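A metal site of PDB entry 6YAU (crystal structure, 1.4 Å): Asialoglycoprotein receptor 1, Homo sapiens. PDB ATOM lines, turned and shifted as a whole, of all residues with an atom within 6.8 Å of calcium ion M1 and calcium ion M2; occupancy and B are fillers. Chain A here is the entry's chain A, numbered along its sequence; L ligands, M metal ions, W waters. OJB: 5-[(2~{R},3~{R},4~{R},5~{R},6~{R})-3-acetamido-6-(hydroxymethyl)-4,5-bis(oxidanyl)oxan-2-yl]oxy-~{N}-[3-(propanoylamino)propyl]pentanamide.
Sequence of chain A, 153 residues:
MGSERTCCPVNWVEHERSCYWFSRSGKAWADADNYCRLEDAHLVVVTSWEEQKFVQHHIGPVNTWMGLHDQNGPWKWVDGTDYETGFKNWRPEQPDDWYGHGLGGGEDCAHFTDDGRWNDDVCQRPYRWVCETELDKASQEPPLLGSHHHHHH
NH2 of Arg 91 is in hydrogen-bond range of O30 of the ligand, 2.9 Å away.
Calcium ion M2 is bound by OD1 of Asp 120 (2.3 Å), OE2 of Glu 107 (2.4 Å), OD1 of Asn 119 (2.4 Å), OD1 of Asp 96 (2.5 Å), OE1 of Gln 94 (2.5 Å), O of Asp 120 (2.5 Å), O25 of the ligand (2.5 Å) and O26 of the ligand (2.6 Å).
Calcium ion M2 has eight donor atoms within binding distance.
Within 4 Å of calcium ion M2: Gln 94, Asp 96, Glu 107, Asn 119 and Asp 120.
The nearest printed residue that does not touch calcium ion M2 is Trp 98 (4.7 Å).
The indole nitrogen (NE1) of Trp 75 sits close to the side-chain carboxylate (OD2) of Asp 70, at 3.4 Å.
The backbone carbonyl oxygen (O) of Asn 119 is in hydrogen-bond range of the backbone NH (N) of His 111 (2.9 Å).
The backbone carbonyl oxygen (O) of Asp 121 sits at hydrogen-bond distance from the backbone NH (N) of Asp 108 (3.2 Å).
The side-chain carboxylate (OD1) of Asp 96 lies close to the backbone NH (N) of Trp 98 (3.4 Å).
The side-chain carboxylate of Asp 120 lies within hydrogen-bond range of the backbone NH of Asp 97 (2.7 Å).
The side-chain carboxylate (OE2) of Glu 107 sits close to the backbone NH (N) of Trp 98 (3.3 Å).
The side-chain amide nitrogen (NE2) of Gln 94 lies close to the guanidinium group (NH2) of Arg 91.
Calcium ion M1 is bound by water W2, OD2 of Asp 70, OD1 of Asp 70, OD1 of Asp 97, OD1 of Asp 108, water W3, water W1 and O of Glu 107.
Calcium ion M1 has eight donor atoms within binding distance.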
ATOM      1  N   HIS A  69       2.748 -31.489  16.907  1.00  0.00           N
ATOM      2  CA  HIS A  69       2.559 -30.058  16.694  1.00  0.00           C
ATOM      3  C   HIS A  69       1.246 -29.568  17.272  1.00  0.00           C
ATOM      4  O   HIS A  69       0.351 -30.377  17.517  1.00  0.00           O
ATOM      5  CB  HIS A  69       2.616 -29.745  15.182  1.00  0.00           C
ATOM      6  CG  HIS A  69       1.400 -30.233  14.457  1.00  0.00           C
ATOM      7  ND1 HIS A  69       0.293 -29.430  14.291  1.00  0.00           N
ATOM      8  CD2 HIS A  69       1.116 -31.480  13.993  1.00  0.00           C
ATOM      9  CE1 HIS A  69      -0.599 -30.176  13.664  1.00  0.00           C
ATOM     10  NE2 HIS A  69      -0.141 -31.410  13.433  1.00  0.00           N
ATOM     11  N   ASP A  70       1.141 -28.263  17.490  1.00  0.00           N
ATOM     12  CA  ASP A  70      -0.095 -27.618  17.950  1.00  0.00           C
ATOM     13  C   ASP A  70      -0.443 -26.383  17.102  1.00  0.00           C
ATOM     14  O   ASP A  70      -0.956 -25.414  17.631  1.00  0.00           O
ATOM     15  CB  ASP A  70      -0.081 -27.315  19.467  1.00  0.00           C
ATOM     16  CG  ASP A  70       0.728 -26.103  19.890  1.00  0.00           C
ATOM     17  OD1 ASP A  70       1.608 -25.683  19.134  1.00  0.00           O
ATOM     18  OD2 ASP A  70       0.487 -25.578  21.003  1.00  0.00           O
ATOM     19  N   GLN A  71      -0.288 -26.625  15.779  1.00  0.00           N
ATOM     20  CA  GLN A  71      -0.648 -25.752  14.701  1.00  0.00           C
ATOM     21  C   GLN A  71      -2.129 -25.932  14.533  1.00  0.00           C
ATOM     22  O   GLN A  71      -2.665 -27.006  14.273  1.00  0.00           O
ATOM     23  CB  GLN A  71       0.101 -26.080  13.403  1.00  0.00           C
ATOM     24  CG  GLN A  71       1.588 -25.705  13.450  1.00  0.00           C
ATOM     25  CD  GLN A  71       2.396 -26.413  12.391  1.00  0.00           C
ATOM     26  OE1 GLN A  71       2.243 -27.613  12.150  1.00  0.00           O
ATOM     27  NE2 GLN A  71       3.296 -25.688  11.743  1.00  0.00           N
ATOM     28  N   GLY A  73      -4.773 -25.650  16.935  1.00  0.00           N
ATOM     29  CA  GLY A  73      -5.521 -26.557  17.787  1.00  0.00           C
ATOM     30  C   GLY A  73      -4.678 -27.079  18.932  1.00  0.00           C
ATOM     31  O   GLY A  73      -3.602 -26.544  19.185  1.00  0.00           O
ATOM     32  N   TRP A  75      -2.176 -29.963  21.045  1.00  0.00           N
ATOM     33  CA  TRP A  75      -1.061 -30.807  20.617  1.00  0.00           C
ATOM     34  C   TRP A  75      -1.579 -32.095  20.029  1.00  0.00           C
ATOM     35  O   TRP A  75      -2.454 -32.735  20.627  1.00  0.00           O
ATOM     36  CB  TRP A  75      -0.111 -31.101  21.787  1.00  0.00           C
ATOM     37  CG  TRP A  75       0.777 -29.937  22.120  1.00  0.00           C
ATOM     38  CD1 TRP A  75       0.594 -29.008  23.107  1.00  0.00           C
ATOM     39  CD2 TRP A  75       1.958 -29.555  21.424  1.00  0.00           C
ATOM     40  NE1 TRP A  75       1.582 -28.057  23.054  1.00  0.00           N
ATOM     41  CE2 TRP A  75       2.433 -28.364  22.002  1.00  0.00           C
ATOM     42  CE3 TRP A  75       2.648 -30.087  20.310  1.00  0.00           C
ATOM     43  CZ2 TRP A  75       3.607 -27.734  21.572  1.00  0.00           C
ATOM     44  CZ3 TRP A  75       3.801 -29.450  19.870  1.00  0.00           C
ATOM     45  CH2 TRP A  75       4.239 -28.264  20.463  1.00  0.00           C
ATOM     46  N   ARG A  91      11.198 -31.332  28.020  1.00  0.00           N
ATOM     47  CA  ARG A  91      12.172 -30.812  28.966  1.00  0.00           C
ATOM     48  C   ARG A  91      11.325 -30.069  30.013  1.00  0.00           C
ATOM     49  O   ARG A  91      10.353 -29.405  29.627  1.00  0.00           O
ATOM     50  CB  ARG A  91      13.130 -29.816  28.301  1.00  0.00           C
ATOM     51  CG  ARG A  91      14.185 -29.254  29.283  1.00  0.00           C
ATOM     52  CD  ARG A  91      15.280 -28.490  28.603  1.00  0.00           C
ATOM     53  NE  ARG A  91      14.798 -27.238  28.036  1.00  0.00           N
ATOM     54  CZ  ARG A  91      15.055 -26.820  26.802  1.00  0.00           C
ATOM     55  NH1 ARG A  91      15.792 -27.561  25.981  1.00  0.00           N
ATOM     56  NH2 ARG A  91      14.595 -25.647  26.386  1.00  0.00           N
ATOM     57  N   GLU A  93       9.408 -27.475  32.071  1.00  0.00           N
ATOM     58  CA  GLU A  93       9.033 -26.099  31.712  1.00  0.00           C
ATOM     59  C   GLU A  93       8.680 -25.987  30.228  1.00  0.00           C
ATOM     60  O   GLU A  93       8.397 -24.889  29.766  1.00  0.00           O
ATOM     61  CB  GLU A  93      10.052 -25.019  32.156  1.00  0.00           C
ATOM     62  CG  GLU A  93      10.340 -25.040  33.654  1.00  0.00           C
ATOM     63  CD  GLU A  93      10.858 -23.741  34.228  1.00  0.00           C
ATOM     64  OE1 GLU A  93      10.084 -22.762  34.314  1.00  0.00           O
ATOM     65  OE2 GLU A  93      12.050 -23.696  34.603  1.00  0.00           O
ATOM     66  N   GLN A  94       8.662 -27.121  29.503  1.00  0.00           N
ATOM     67  CA  GLN A  94       8.222 -27.124  28.116  1.00  0.00           C
ATOM     68  C   GLN A  94       6.975 -28.020  28.065  1.00  0.00           C
ATOM     69  O   GLN A  94       6.839 -28.910  28.921  1.00  0.00           O
ATOM     70  CB  GLN A  94       9.324 -27.629  27.160  1.00  0.00           C
ATOM     71  CG  GLN A  94      10.639 -26.845  27.245  1.00  0.00           C
ATOM     72  CD  GLN A  94      10.594 -25.399  26.755  1.00  0.00           C
ATOM     73  OE1 GLN A  94       9.693 -24.972  26.005  1.00  0.00           O
ATOM     74  NE2 GLN A  94      11.587 -24.616  27.169  1.00  0.00           N
ATOM     75  N   PRO A  95       6.055 -27.825  27.104  1.00  0.00           N
ATOM     76  CA  PRO A  95       6.055 -26.780  26.061  1.00  0.00           C
ATOM     77  C   PRO A  95       5.688 -25.406  26.634  1.00  0.00           C
ATOM     78  O   PRO A  95       4.863 -25.345  27.517  1.00  0.00           O
ATOM     79  CB  PRO A  95       4.999 -27.281  25.074  1.00  0.00           C
ATOM     80  CG  PRO A  95       4.035 -28.098  25.888  1.00  0.00           C
ATOM     81  CD  PRO A  95       4.813 -28.630  27.079  1.00  0.00           C
ATOM     82  N   ASP A  96       6.313 -24.319  26.164  1.00  0.00           N
ATOM     83  CA  ASP A  96       6.000 -22.998  26.715  1.00  0.00           C
ATOM     84  C   ASP A  96       5.357 -22.035  25.697  1.00  0.00           C
ATOM     85  O   ASP A  96       5.001 -20.930  26.076  1.00  0.00           O
ATOM     86  CB  ASP A  96       7.245 -22.363  27.357  1.00  0.00           C
ATOM     87  CG  ASP A  96       8.398 -22.153  26.400  1.00  0.00           C
ATOM     88  OD1 ASP A  96       8.274 -22.549  25.241  1.00  0.00           O
ATOM     89  OD2 ASP A  96       9.423 -21.587  26.811  1.00  0.00           O
ATOM     90  N   ASP A  97       5.215 -22.441  24.427  1.00  0.00           N
ATOM     91  CA  ASP A  97       4.626 -21.571  23.378  1.00  0.00           C
ATOM     92  C   ASP A  97       5.280 -20.184  23.404  1.00  0.00           C
ATOM     93  O   ASP A  97       4.578 -19.173  23.323  1.00  0.00           O
ATOM     94  CB  ASP A  97       3.098 -21.420  23.573  1.00  0.00           C
ATOM     95  CG  ASP A  97       2.367 -20.962  22.329  1.00  0.00           C
ATOM     96  OD1 ASP A  97       2.665 -21.489  21.225  1.00  0.00           O
ATOM     97  OD2 ASP A  97       1.481 -20.071  22.466  1.00  0.00           O
ATOM     98  N   TRP A  98       6.608 -20.147  23.521  1.00  0.00           N
ATOM     99  CA  TRP A  98       7.378 -18.896  23.659  1.00  0.00           C
ATOM    100  C   TRP A  98       7.194 -17.886  22.529  1.00  0.00           C
ATOM    101  O   TRP A  98       7.244 -18.256  21.341  1.00  0.00           O
ATOM    102  CB  TRP A  98       8.854 -19.222  23.851  1.00  0.00           C
ATOM    103  CG  TRP A  98       9.759 -18.108  24.300  1.00  0.00           C
ATOM    104  CD1 TRP A  98       9.582 -17.280  25.377  1.00  0.00           C
ATOM    105  CD2 TRP A  98      11.080 -17.831  23.809  1.00  0.00           C
ATOM    106  NE1 TRP A  98      10.677 -16.468  25.543  1.00  0.00           N
ATOM    107  CE2 TRP A  98      11.637 -16.812  24.614  1.00  0.00           C
ATOM    108  CE3 TRP A  98      11.825 -18.314  22.712  1.00  0.00           C
ATOM    109  CZ2 TRP A  98      12.895 -16.254  24.353  1.00  0.00           C
ATOM    110  CZ3 TRP A  98      13.106 -17.803  22.488  1.00  0.00           C
ATOM    111  CH2 TRP A  98      13.632 -16.800  23.317  1.00  0.00           C
ATOM    112  N   GLY A 106       3.884 -17.961  18.531  1.00  0.00           N
ATOM    113  CA  GLY A 106       4.429 -18.707  19.650  1.00  0.00           C
ATOM    114  C   GLY A 106       5.386 -19.744  19.117  1.00  0.00           C
ATOM    115  O   GLY A 106       6.254 -19.426  18.306  1.00  0.00           O
ATOM    116  N   GLU A 107       5.203 -20.999  19.558  1.00  0.00           N
ATOM    117  CA  GLU A 107       6.039 -22.126  19.132  1.00  0.00           C
ATOM    118  C   GLU A 107       5.105 -23.298  18.956  1.00  0.00           C
ATOM    119  O   GLU A 107       4.419 -23.703  19.879  1.00  0.00           O
ATOM    120  CB  GLU A 107       7.124 -22.409  20.180  1.00  0.00           C
ATOM    121  CG  GLU A 107       8.230 -21.352  20.243  1.00  0.00           C
ATOM    122  CD  GLU A 107       9.282 -21.620  21.301  1.00  0.00           C
ATOM    123  OE1 GLU A 107      10.474 -21.334  21.063  1.00  0.00           O
ATOM    124  OE2 GLU A 107       8.909 -22.153  22.369  1.00  0.00           O
ATOM    125  N   ASP A 108       5.036 -23.837  17.758  1.00  0.00           N
ATOM    126  CA  ASP A 108       4.018 -24.838  17.503  1.00  0.00           C
ATOM    127  C   ASP A 108       4.531 -26.182  17.033  1.00  0.00           C
ATOM    128  O   ASP A 108       3.707 -27.055  16.764  1.00  0.00           O
ATOM    129  CB  ASP A 108       3.007 -24.282  16.477  1.00  0.00           C
ATOM    130  CG  ASP A 108       2.209 -23.080  16.954  1.00  0.00           C
ATOM    131  OD1 ASP A 108       2.147 -22.844  18.200  1.00  0.00           O
ATOM    132  OD2 ASP A 108       1.662 -22.368  16.099  1.00  0.00           O
ATOM    133  N   CYS A 109       5.860 -26.394  16.962  1.00  0.00           N
ATOM    134  CA  CYS A 109       6.369 -27.658  16.487  1.00  0.00           C
ATOM    135  C   CYS A 109       7.331 -28.272  17.468  1.00  0.00           C
ATOM    136  O   CYS A 109       8.237 -27.572  17.916  1.00  0.00           O
ATOM    137  CB  CYS A 109       7.007 -27.486  15.125  1.00  0.00           C
ATOM    138  SG  CYS A 109       5.830 -27.061  13.810  1.00  0.00           S
ATOM    139  N   HIS A 111      10.443 -30.773  18.789  1.00  0.00           N
ATOM    140  CA  HIS A 111      11.693 -31.375  18.340  1.00  0.00           C
ATOM    141  C   HIS A 111      12.428 -32.023  19.499  1.00  0.00           C
ATOM    142  O   HIS A 111      12.196 -31.680  20.672  1.00  0.00           O
ATOM    143  CB  HIS A 111      12.595 -30.346  17.639  1.00  0.00           C
ATOM    144  CG  HIS A 111      13.106 -29.265  18.533  1.00  0.00           C
ATOM    145  ND1 HIS A 111      14.430 -29.222  18.987  1.00  0.00           N
ATOM    146  CD2 HIS A 111      12.463 -28.162  18.996  1.00  0.00           C
ATOM    147  CE1 HIS A 111      14.524 -28.128  19.723  1.00  0.00           C
ATOM    148  NE2 HIS A 111      13.374 -27.466  19.774  1.00  0.00           N
ATOM    149  N   ASN A 119      11.212 -30.067  23.098  1.00  0.00           N
ATOM    150  CA  ASN A 119      10.944 -28.632  23.188  1.00  0.00           C
ATOM    151  C   ASN A 119      10.011 -28.245  22.045  1.00  0.00           C
ATOM    152  O   ASN A 119      10.050 -28.860  20.961  1.00  0.00           O
ATOM    153  CB  ASN A 119      12.237 -27.828  23.077  1.00  0.00           C
ATOM    154  CG  ASN A 119      11.997 -26.316  23.016  1.00  0.00           C
ATOM    155  OD1 ASN A 119      11.346 -25.735  23.888  1.00  0.00           O
ATOM    156  ND2 ASN A 119      12.472 -25.667  21.976  1.00  0.00           N
ATOM    157  N   ASP A 120       9.110 -27.307  22.325  1.00  0.00           N
ATOM    158  CA  ASP A 120       8.329 -26.747  21.256  1.00  0.00           C
ATOM    159  C   ASP A 120       9.132 -25.553  20.710  1.00  0.00           C
ATOM    160  O   ASP A 120       9.697 -24.745  21.466  1.00  0.00           O
ATOM    161  CB  ASP A 120       6.913 -26.311  21.715  1.00  0.00           C
ATOM    162  CG  ASP A 120       6.801 -25.293  22.852  1.00  0.00           C
ATOM    163  OD1 ASP A 120       7.808 -25.129  23.633  1.00  0.00           O
ATOM    164  OD2 ASP A 120       5.708 -24.684  22.990  1.00  0.00           O
ATOM    165  N   ASP A 121       9.106 -25.417  19.371  1.00  0.00           N
ATOM    166  CA  ASP A 121       9.863 -24.339  18.757  1.00  0.00           C
ATOM    167  C   ASP A 121       9.158 -23.776  17.535  1.00  0.00           C
ATOM    168  O   ASP A 121       8.111 -24.274  17.108  1.00  0.00           O
ATOM    169  CB  ASP A 121      11.313 -24.853  18.429  1.00  0.00           C
ATOM    170  CG  ASP A 121      12.442 -23.803  18.488  1.00  0.00           C
ATOM    171  OD1 ASP A 121      13.615 -24.194  18.779  1.00  0.00           O
ATOM    172  OD2 ASP A 121      12.153 -22.618  18.257  1.00  0.00           O
HETATM  173  C1  OJB L   1      19.150 -22.593  22.539  1.00  0.00           C
HETATM  174  C12 OJB L   1      19.182 -22.266  24.017  1.00  0.00           C
HETATM  175  C13 OJB L   1      18.651 -23.386  24.916  1.00  0.00           C
HETATM  176  C14 OJB L   1      18.064 -22.893  26.232  1.00  0.00           C
HETATM  177  C15 OJB L   1      16.800 -22.062  26.078  1.00  0.00           C
HETATM  178  C19 OJB L   1      12.939 -20.647  25.365  1.00  0.00           C
HETATM  179  C20 OJB L   1      11.981 -21.418  24.455  1.00  0.00           C
HETATM  180  C21 OJB L   1      12.752 -22.069  23.306  1.00  0.00           C
HETATM  181  C22 OJB L   1      13.952 -22.864  23.824  1.00  0.00           C
HETATM  182  N2  OJB L   1      18.597 -21.671  21.755  1.00  0.00           N
HETATM  183  O3  OJB L   1      19.601 -23.654  22.112  1.00  0.00           O
HETATM  184  O16 OJB L   1      15.824 -22.819  25.352  1.00  0.00           O
HETATM  185  C17 OJB L   1      14.782 -22.051  24.822  1.00  0.00           C
HETATM  186  O18 OJB L   1      13.963 -21.547  25.858  1.00  0.00           O
HETATM  187  C23 OJB L   1      12.245 -20.026  26.561  1.00  0.00           C
HETATM  188  O24 OJB L   1      13.134 -19.192  27.305  1.00  0.00           O
HETATM  189  O25 OJB L   1      11.299 -22.416  25.206  1.00  0.00           O
HETATM  190  O26 OJB L   1      11.899 -22.949  22.602  1.00  0.00           O
HETATM  191  N27 OJB L   1      14.769 -23.337  22.724  1.00  0.00           N
HETATM  192  C28 OJB L   1      15.364 -24.534  22.688  1.00  0.00           C
HETATM  193  C29 OJB L   1      16.107 -24.864  21.432  1.00  0.00           C
HETATM  194  O30 OJB L   1      15.275 -25.338  23.625  1.00  0.00           O
HETATM  195 CA    CA M   1       1.958 -23.733  20.536  1.00  0.00          CA
HETATM  196 CA    CA M   2       9.770 -23.869  23.816  1.00  0.00          CA
HETATM  197  O   HOH W   1      -0.221 -22.810  19.612  1.00  0.00           O
HETATM  198  O   HOH W   2       3.078 -24.448  22.413  1.00  0.00           O
HETATM  199  O   HOH W   3       0.202 -23.009  22.214  1.00  0.00           O
